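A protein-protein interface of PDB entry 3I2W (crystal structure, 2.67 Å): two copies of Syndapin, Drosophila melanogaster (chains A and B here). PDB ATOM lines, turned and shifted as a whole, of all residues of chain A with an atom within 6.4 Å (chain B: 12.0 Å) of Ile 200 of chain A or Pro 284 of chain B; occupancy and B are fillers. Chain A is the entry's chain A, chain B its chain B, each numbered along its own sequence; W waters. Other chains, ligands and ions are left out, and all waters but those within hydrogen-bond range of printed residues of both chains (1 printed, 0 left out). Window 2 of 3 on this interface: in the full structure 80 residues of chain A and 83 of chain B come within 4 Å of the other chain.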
ATOM      1  N   TRP A 130     -16.504   3.258  21.701  1.00  0.00           N
ATOM      2  CA  TRP A 130     -17.692   3.236  22.519  1.00  0.00           C
ATOM      3  C   TRP A 130     -18.014   1.857  23.066  1.00  0.00           C
ATOM      4  O   TRP A 130     -18.532   1.709  24.177  1.00  0.00           O
ATOM      5  CB  TRP A 130     -18.853   3.748  21.662  1.00  0.00           C
ATOM      6  CG  TRP A 130     -20.130   3.922  22.356  1.00  0.00           C
ATOM      7  CD1 TRP A 130     -20.548   5.011  23.021  1.00  0.00           C
ATOM      8  CD2 TRP A 130     -21.175   2.960  22.452  1.00  0.00           C
ATOM      9  NE1 TRP A 130     -21.795   4.784  23.565  1.00  0.00           N
ATOM     10  CE2 TRP A 130     -22.201   3.531  23.200  1.00  0.00           C
ATOM     11  CE3 TRP A 130     -21.344   1.664  21.958  1.00  0.00           C
ATOM     12  CZ2 TRP A 130     -23.382   2.870  23.450  1.00  0.00           C
ATOM     13  CZ3 TRP A 130     -22.494   1.001  22.221  1.00  0.00           C
ATOM     14  CH2 TRP A 130     -23.504   1.589  22.973  1.00  0.00           C
ATOM     15  N   ALA A 131     -17.704   0.843  22.268  1.00  0.00           N
ATOM     16  CA  ALA A 131     -18.077  -0.536  22.569  1.00  0.00           C
ATOM     17  C   ALA A 131     -17.239  -1.020  23.736  1.00  0.00           C
ATOM     18  O   ALA A 131     -17.627  -1.955  24.463  1.00  0.00           O
ATOM     19  CB  ALA A 131     -17.814  -1.400  21.361  1.00  0.00           C
ATOM     20  N   LEU A 133     -15.917   1.194  26.058  1.00  0.00           N
ATOM     21  CA  LEU A 133     -16.538   1.788  27.240  1.00  0.00           C
ATOM     22  C   LEU A 133     -17.750   0.982  27.671  1.00  0.00           C
ATOM     23  O   LEU A 133     -18.053   0.901  28.832  1.00  0.00           O
ATOM     24  CB  LEU A 133     -16.895   3.244  27.027  1.00  0.00           C
ATOM     25  CG  LEU A 133     -15.751   4.083  26.472  1.00  0.00           C
ATOM     26  CD1 LEU A 133     -16.093   5.537  26.472  1.00  0.00           C
ATOM     27  CD2 LEU A 133     -14.541   3.905  27.323  1.00  0.00           C
ATOM     28  N   LEU A 134     -18.434   0.337  26.744  1.00  0.00           N
ATOM     29  CA  LEU A 134     -19.664  -0.317  27.127  1.00  0.00           C
ATOM     30  C   LEU A 134     -19.272  -1.587  27.801  1.00  0.00           C
ATOM     31  O   LEU A 134     -20.008  -2.080  28.663  1.00  0.00           O
ATOM     32  CB  LEU A 134     -20.569  -0.605  25.930  1.00  0.00           C
ATOM     33  CG  LEU A 134     -21.898  -1.175  26.433  1.00  0.00           C
ATOM     34  CD1 LEU A 134     -23.091  -0.209  26.275  1.00  0.00           C
ATOM     35  CD2 LEU A 134     -22.171  -2.548  25.784  1.00  0.00           C
ATOM     36  N   ALA A 135     -18.107  -2.106  27.396  1.00  0.00           N
ATOM     37  CA  ALA A 135     -17.543  -3.361  27.941  1.00  0.00           C
ATOM     38  C   ALA A 135     -17.152  -3.147  29.398  1.00  0.00           C
ATOM     39  O   ALA A 135     -17.526  -3.957  30.261  1.00  0.00           O
ATOM     40  CB  ALA A 135     -16.326  -3.843  27.125  1.00  0.00           C
ATOM     41  N   VAL A 137     -18.456  -0.538  31.318  1.00  0.00           N
ATOM     42  CA  VAL A 137     -19.686  -0.519  32.082  1.00  0.00           C
ATOM     43  C   VAL A 137     -20.141  -1.953  32.461  1.00  0.00           C
ATOM     44  O   VAL A 137     -20.544  -2.207  33.595  1.00  0.00           O
ATOM     45  CB  VAL A 137     -20.785   0.283  31.389  1.00  0.00           C
ATOM     46  CG1 VAL A 137     -22.118   0.128  32.133  1.00  0.00           C
ATOM     47  CG2 VAL A 137     -20.376   1.726  31.322  1.00  0.00           C
ATOM     48  N   GLU A 138     -20.058  -2.893  31.526  1.00  0.00           N
ATOM     49  CA  GLU A 138     -20.644  -4.207  31.752  1.00  0.00           C
ATOM     50  C   GLU A 138     -19.973  -5.027  32.851  1.00  0.00           C
ATOM     51  O   GLU A 138     -20.667  -5.699  33.632  1.00  0.00           O
ATOM     52  CB  GLU A 138     -20.722  -4.991  30.446  1.00  0.00           C
ATOM     53  CG  GLU A 138     -21.917  -4.591  29.583  1.00  0.00           C
ATOM     54  CD  GLU A 138     -23.235  -4.597  30.369  1.00  0.00           C
ATOM     55  OE1 GLU A 138     -23.842  -5.684  30.530  1.00  0.00           O
ATOM     56  OE2 GLU A 138     -23.665  -3.509  30.828  1.00  0.00           O
ATOM     57  N   LYS A 141     -20.604  -3.267  36.244  1.00  0.00           N
ATOM     58  CA  LYS A 141     -21.964  -3.594  36.652  1.00  0.00           C
ATOM     59  C   LYS A 141     -21.989  -4.960  37.310  1.00  0.00           C
ATOM     60  O   LYS A 141     -22.665  -5.130  38.311  1.00  0.00           O
ATOM     61  CB  LYS A 141     -22.954  -3.502  35.479  1.00  0.00           C
ATOM     62  CG  LYS A 141     -23.909  -4.702  35.294  1.00  0.00           C
ATOM     63  CD  LYS A 141     -25.338  -4.310  34.871  1.00  0.00           C
ATOM     64  CE  LYS A 141     -25.374  -3.058  33.986  1.00  0.00           C
ATOM     65  NZ  LYS A 141     -26.521  -3.073  33.026  1.00  0.00           N
ATOM     66  N   GLN A 195     -18.516   5.634  37.166  1.00  0.00           N
ATOM     67  CA  GLN A 195     -17.465   6.448  36.621  1.00  0.00           C
ATOM     68  C   GLN A 195     -17.221   5.954  35.232  1.00  0.00           C
ATOM     69  O   GLN A 195     -16.756   6.686  34.370  1.00  0.00           O
ATOM     70  CB  GLN A 195     -16.207   6.290  37.464  1.00  0.00           C
ATOM     71  CG  GLN A 195     -15.212   7.460  37.363  1.00  0.00           C
ATOM     72  CD  GLN A 195     -14.126   7.415  38.462  1.00  0.00           C
ATOM     73  OE1 GLN A 195     -14.210   6.625  39.418  1.00  0.00           O
ATOM     74  NE2 GLN A 195     -13.107   8.266  38.323  1.00  0.00           N
ATOM     75  N   ALA A 196     -17.506   4.675  35.049  1.00  0.00           N
ATOM     76  CA  ALA A 196     -17.534   4.057  33.755  1.00  0.00           C
ATOM     77  C   ALA A 196     -18.721   4.692  32.995  1.00  0.00           C
ATOM     78  O   ALA A 196     -18.589   5.224  31.868  1.00  0.00           O
ATOM     79  CB  ALA A 196     -17.724   2.570  33.918  1.00  0.00           C
ATOM     80  N   ILE A 197     -19.867   4.648  33.661  1.00  0.00           N
ATOM     81  CA  ILE A 197     -21.007   5.390  33.257  1.00  0.00           C
ATOM     82  C   ILE A 197     -20.681   6.860  32.927  1.00  0.00           C
ATOM     83  O   ILE A 197     -20.970   7.327  31.831  1.00  0.00           O
ATOM     84  CB  ILE A 197     -22.065   5.315  34.311  1.00  0.00           C
ATOM     85  CG1 ILE A 197     -22.725   3.941  34.259  1.00  0.00           C
ATOM     86  CG2 ILE A 197     -23.057   6.446  34.092  1.00  0.00           C
ATOM     87  CD1 ILE A 197     -24.084   3.888  34.903  1.00  0.00           C
ATOM     88  N   ALA A 198     -20.076   7.603  33.840  1.00  0.00           N
ATOM     89  CA  ALA A 198     -19.829   9.006  33.533  1.00  0.00           C
ATOM     90  C   ALA A 198     -18.989   9.120  32.252  1.00  0.00           C
ATOM     91  O   ALA A 198     -19.069  10.133  31.517  1.00  0.00           O
ATOM     92  CB  ALA A 198     -19.156   9.715  34.709  1.00  0.00           C
ATOM     93  N   GLU A 199     -18.192   8.075  31.998  1.00  0.00           N
ATOM     94  CA  GLU A 199     -17.177   8.162  30.962  1.00  0.00           C
ATOM     95  C   GLU A 199     -17.781   7.922  29.595  1.00  0.00           C
ATOM     96  O   GLU A 199     -17.533   8.678  28.646  1.00  0.00           O
ATOM     97  CB  GLU A 199     -16.023   7.200  31.172  1.00  0.00           C
ATOM     98  CG  GLU A 199     -14.764   7.837  30.597  1.00  0.00           C
ATOM     99  CD  GLU A 199     -13.702   6.846  30.103  1.00  0.00           C
ATOM    100  OE1 GLU A 199     -13.206   6.016  30.918  1.00  0.00           O
ATOM    101  OE2 GLU A 199     -13.332   6.926  28.898  1.00  0.00           O
ATOM    102  N   ILE A 200     -18.562   6.844  29.523  1.00  0.00           N
ATOM    103  CA  ILE A 200     -19.332   6.527  28.358  1.00  0.00           C
ATOM    104  C   ILE A 200     -20.234   7.701  28.133  1.00  0.00           C
ATOM    105  O   ILE A 200     -20.147   8.315  27.079  1.00  0.00           O
ATOM    106  CB  ILE A 200     -20.082   5.178  28.474  1.00  0.00           C
ATOM    107  CG1 ILE A 200     -20.200   4.562  27.075  1.00  0.00           C
ATOM    108  CG2 ILE A 200     -21.414   5.291  29.272  1.00  0.00           C
ATOM    109  CD1 ILE A 200     -20.978   3.200  26.993  1.00  0.00           C
ATOM    110  N   THR A 201     -21.031   8.079  29.129  1.00  0.00           N
ATOM    111  CA  THR A 201     -21.954   9.196  28.937  1.00  0.00           C
ATOM    112  C   THR A 201     -21.261  10.369  28.270  1.00  0.00           C
ATOM    113  O   THR A 201     -21.884  11.088  27.496  1.00  0.00           O
ATOM    114  CB  THR A 201     -22.661   9.592  30.223  1.00  0.00           C
ATOM    115  OG1 THR A 201     -23.418   8.470  30.657  1.00  0.00           O
ATOM    116  CG2 THR A 201     -23.656  10.722  30.014  1.00  0.00           C
ATOM    117  N   LYS A 202     -19.961  10.523  28.493  1.00  0.00           N
ATOM    118  CA  LYS A 202     -19.241  11.626  27.907  1.00  0.00           C
ATOM    119  C   LYS A 202     -18.854  11.349  26.456  1.00  0.00           C
ATOM    120  O   LYS A 202     -18.635  12.292  25.703  1.00  0.00           O
ATOM    121  CB  LYS A 202     -17.988  11.895  28.718  1.00  0.00           C
ATOM    122  CG  LYS A 202     -17.820  13.379  29.147  1.00  0.00           C
ATOM    123  CD  LYS A 202     -16.315  13.760  29.333  1.00  0.00           C
ATOM    124  CE  LYS A 202     -15.759  14.389  28.012  1.00  0.00           C
ATOM    125  NZ  LYS A 202     -14.263  14.584  28.012  1.00  0.00           N
ATOM    126  N   TYR A 203     -18.764  10.078  26.057  1.00  0.00           N
ATOM    127  CA  TYR A 203     -18.381   9.735  24.705  1.00  0.00           C
ATOM    128  C   TYR A 203     -19.583   9.742  23.731  1.00  0.00           C
ATOM    129  O   TYR A 203     -19.452  10.067  22.533  1.00  0.00           O
ATOM    130  CB  TYR A 203     -17.699   8.402  24.702  1.00  0.00           C
ATOM    131  CG  TYR A 203     -16.984   8.112  23.424  1.00  0.00           C
ATOM    132  CD1 TYR A 203     -15.861   8.826  23.086  1.00  0.00           C
ATOM    133  CD2 TYR A 203     -17.413   7.103  22.563  1.00  0.00           C
ATOM    134  CE1 TYR A 203     -15.187   8.571  21.931  1.00  0.00           C
ATOM    135  CE2 TYR A 203     -16.712   6.826  21.397  1.00  0.00           C
ATOM    136  CZ  TYR A 203     -15.595   7.582  21.095  1.00  0.00           C
ATOM    137  OH  TYR A 203     -14.856   7.374  19.964  1.00  0.00           O
ATOM    138  N   ASN A 204     -20.792   9.439  24.250  1.00  0.00           N
ATOM    139  CA  ASN A 204     -22.001   9.412  23.459  1.00  0.00           C
ATOM    140  C   ASN A 204     -22.041  10.433  22.373  1.00  0.00           C
ATOM    141  O   ASN A 204     -21.945  10.063  21.211  1.00  0.00           O
ATOM    142  CB  ASN A 204     -23.223   9.461  24.374  1.00  0.00           C
ATOM    143  CG  ASN A 204     -23.227   8.305  25.348  1.00  0.00           C
ATOM    144  OD1 ASN A 204     -22.504   7.306  25.148  1.00  0.00           O
ATOM    145  ND2 ASN A 204     -24.003   8.427  26.409  1.00  0.00           N
ATOM    146  N   SER A 205     -22.043  11.724  22.774  1.00  0.00           N
ATOM    147  CA  SER A 205     -21.963  12.758  21.732  1.00  0.00           C
ATOM    148  C   SER A 205     -21.043  12.361  20.521  1.00  0.00           C
ATOM    149  O   SER A 205     -21.392  12.599  19.347  1.00  0.00           O
ATOM    150  CB  SER A 205     -21.531  14.130  22.311  1.00  0.00           C
ATOM    151  OG  SER A 205     -20.194  14.507  21.871  1.00  0.00           O
ATOM    152  N   ALA B 280     -34.707   4.944  18.886  1.00  0.00           N
ATOM    153  CA  ALA B 280     -34.380   5.248  20.257  1.00  0.00           C
ATOM    154  C   ALA B 280     -33.203   4.395  20.752  1.00  0.00           C
ATOM    155  O   ALA B 280     -32.997   3.297  20.283  1.00  0.00           O
ATOM    156  CB  ALA B 280     -35.561   5.036  21.082  1.00  0.00           C
ATOM    157  N   MET B 281     -32.378   4.934  21.634  1.00  0.00           N
ATOM    158  CA  MET B 281     -31.442   4.160  22.385  1.00  0.00           C
ATOM    159  C   MET B 281     -31.612   4.708  23.751  1.00  0.00           C
ATOM    160  O   MET B 281     -31.659   5.926  23.915  1.00  0.00           O
ATOM    161  CB  MET B 281     -30.043   4.452  21.951  1.00  0.00           C
ATOM    162  CG  MET B 281     -28.975   3.683  22.703  1.00  0.00           C
ATOM    163  SD  MET B 281     -29.181   1.949  22.580  1.00  0.00           S
ATOM    164  CE  MET B 281     -27.499   1.522  22.817  1.00  0.00           C
ATOM    165  N   ASN B 282     -31.751   3.831  24.739  1.00  0.00           N
ATOM    166  CA  ASN B 282     -31.472   4.237  26.125  1.00  0.00           C
ATOM    167  C   ASN B 282     -30.005   3.916  26.361  1.00  0.00           C
ATOM    168  O   ASN B 282     -29.545   2.810  26.193  1.00  0.00           O
ATOM    169  CB  ASN B 282     -32.343   3.459  27.094  1.00  0.00           C
ATOM    170  CG  ASN B 282     -32.512   2.054  26.632  1.00  0.00           C
ATOM    171  OD1 ASN B 282     -31.537   1.452  26.149  1.00  0.00           O
ATOM    172  ND2 ASN B 282     -33.754   1.535  26.675  1.00  0.00           N
ATOM    173  N   TRP B 283     -29.271   4.926  26.734  1.00  0.00           N
ATOM    174  CA  TRP B 283     -27.896   4.769  27.026  1.00  0.00           C
ATOM    175  C   TRP B 283     -27.706   4.045  28.360  1.00  0.00           C
ATOM    176  O   TRP B 283     -28.662   3.876  29.107  1.00  0.00           O
ATOM    177  CB  TRP B 283     -27.354   6.186  26.993  1.00  0.00           C
ATOM    178  CG  TRP B 283     -27.735   6.782  25.674  1.00  0.00           C
ATOM    179  CD1 TRP B 283     -28.791   7.582  25.415  1.00  0.00           C
ATOM    180  CD2 TRP B 283     -27.109   6.520  24.404  1.00  0.00           C
ATOM    181  NE1 TRP B 283     -28.838   7.886  24.075  1.00  0.00           N
ATOM    182  CE2 TRP B 283     -27.822   7.239  23.434  1.00  0.00           C
ATOM    183  CE3 TRP B 283     -26.000   5.754  24.001  1.00  0.00           C
ATOM    184  CZ2 TRP B 283     -27.456   7.244  22.108  1.00  0.00           C
ATOM    185  CZ3 TRP B 283     -25.652   5.749  22.692  1.00  0.00           C
ATOM    186  CH2 TRP B 283     -26.373   6.495  21.754  1.00  0.00           C
ATOM    187  N   PRO B 284     -26.489   3.575  28.672  1.00  0.00           N
ATOM    188  CA  PRO B 284     -26.459   2.922  29.971  1.00  0.00           C
ATOM    189  C   PRO B 284     -26.619   3.873  31.145  1.00  0.00           C
ATOM    190  O   PRO B 284     -26.077   4.973  31.130  1.00  0.00           O
ATOM    191  CB  PRO B 284     -25.076   2.289  30.011  1.00  0.00           C
ATOM    192  CG  PRO B 284     -24.317   2.887  28.885  1.00  0.00           C
ATOM    193  CD  PRO B 284     -25.298   3.259  27.873  1.00  0.00           C
ATOM    194  N   SER B 285     -27.402   3.430  32.133  1.00  0.00           N
ATOM    195  CA  SER B 285     -27.343   3.915  33.517  1.00  0.00           C
ATOM    196  C   SER B 285     -27.446   2.751  34.503  1.00  0.00           C
ATOM    197  O   SER B 285     -27.128   2.937  35.720  1.00  0.00           O
ATOM    198  CB  SER B 285     -28.418   4.957  33.804  1.00  0.00           C
ATOM    199  OG  SER B 285     -28.241   6.067  32.947  1.00  0.00           O
HETATM  200  O   HOH W   1     -24.763   6.479  28.760  1.00  0.00           O
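The backbone carbonyl oxygen (O) of Ile 197 of chain A sits at hydrogen-bond distance from the side-chain hydroxyl (OG1) of Thr 201 of chain A, 2.9 Å away. The backbone carbonyl oxygen of Met 281 of chain B lies within hydrogen-bond range of the indole nitrogen of Trp 283 of chain B (3.4 Å). The indole nitrogen (NE1) of Trp 130 of chain A is in hydrogen-bond range of the side-chain amide oxygen (OD1) of Asn 204 of chain A. The backbone carbonyl oxygen of Ile 200 of chain A sits close to the side-chain amide oxygen of Asn 204 of chain A (3.2 Å).
Among the printed residues, merely in contact across the chains: Trp 130 of chain A with Met 281 of chain B (3.999 Å), Trp 130 of chain A with Trp 283 of chain B (3.7 Å), Ile 197 of chain A with Ser 285 of chain B (3.3 Å), Ile 200 of chain A with Pro 284 of chain B (3.8 Å) and Asn 204 of chain A with Trp 283 of chain B (3.99 Å).
Of the printed residues of chain B, Trp 130 of chain A touches Met 281 (3.999 Å) and Trp 283 (3.7 Å). Ala 131 of chain A touches none of the printed residues of chain B. Leu 133 of chain A touches none of the printed residues of chain B. Val 137 of chain A touches none of the printed residues of chain B. Ile 200 of chain A touches just one residue of chain B: Pro 284 (3.8 Å). No residue of chain B comes within 4 Å of Thr 201 of chain A. Tyr 203 of chain A touches none of the printed residues of chain B. Ser 205 of chain A touches none of the printed residues of chain B. Of the printed residues of chain A, Trp 283 of chain B touches Trp 130 (3.7 Å) and Asn 204 (3.99 Å). Printed residues of chain A within 4 Å of Ser 285 of chain B: Ile 197.
Of the 6 printed residues of chain B, 4 touch a printed residue of chain A. Hydrophobic or aromatic side chains of chain B within 4 Å of the printed part of chain A: Met 281, Trp 283 and Pro 284. Along chain B the printed residues that touch a printed residue of chain A span positions 281 to 285. Hydrophobic or aromatic side chains of chain A that line the printed part of chain B: Trp 130, Ile 197 and Ile 200. Along chain A the printed residues that touch a printed residue of chain B span positions 130 to 204. Among the printed residues, 5 pairs touch across the chains.
No position is printed for both chains. Of the 5 pairs that touch across the chains among the printed residues, none has its exchanged pair printed and touching as well.
Water W1 lies within hydrogen-bond range of the side-chain hydroxyl (OG1) of Thr 201 of chain A (3.1 Å), the backbone carbonyl oxygen (O) of Pro 284 of chain B (3.1 Å) and the side-chain amide nitrogen (ND2) of Asn 204 of chain A (3.1 Å).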
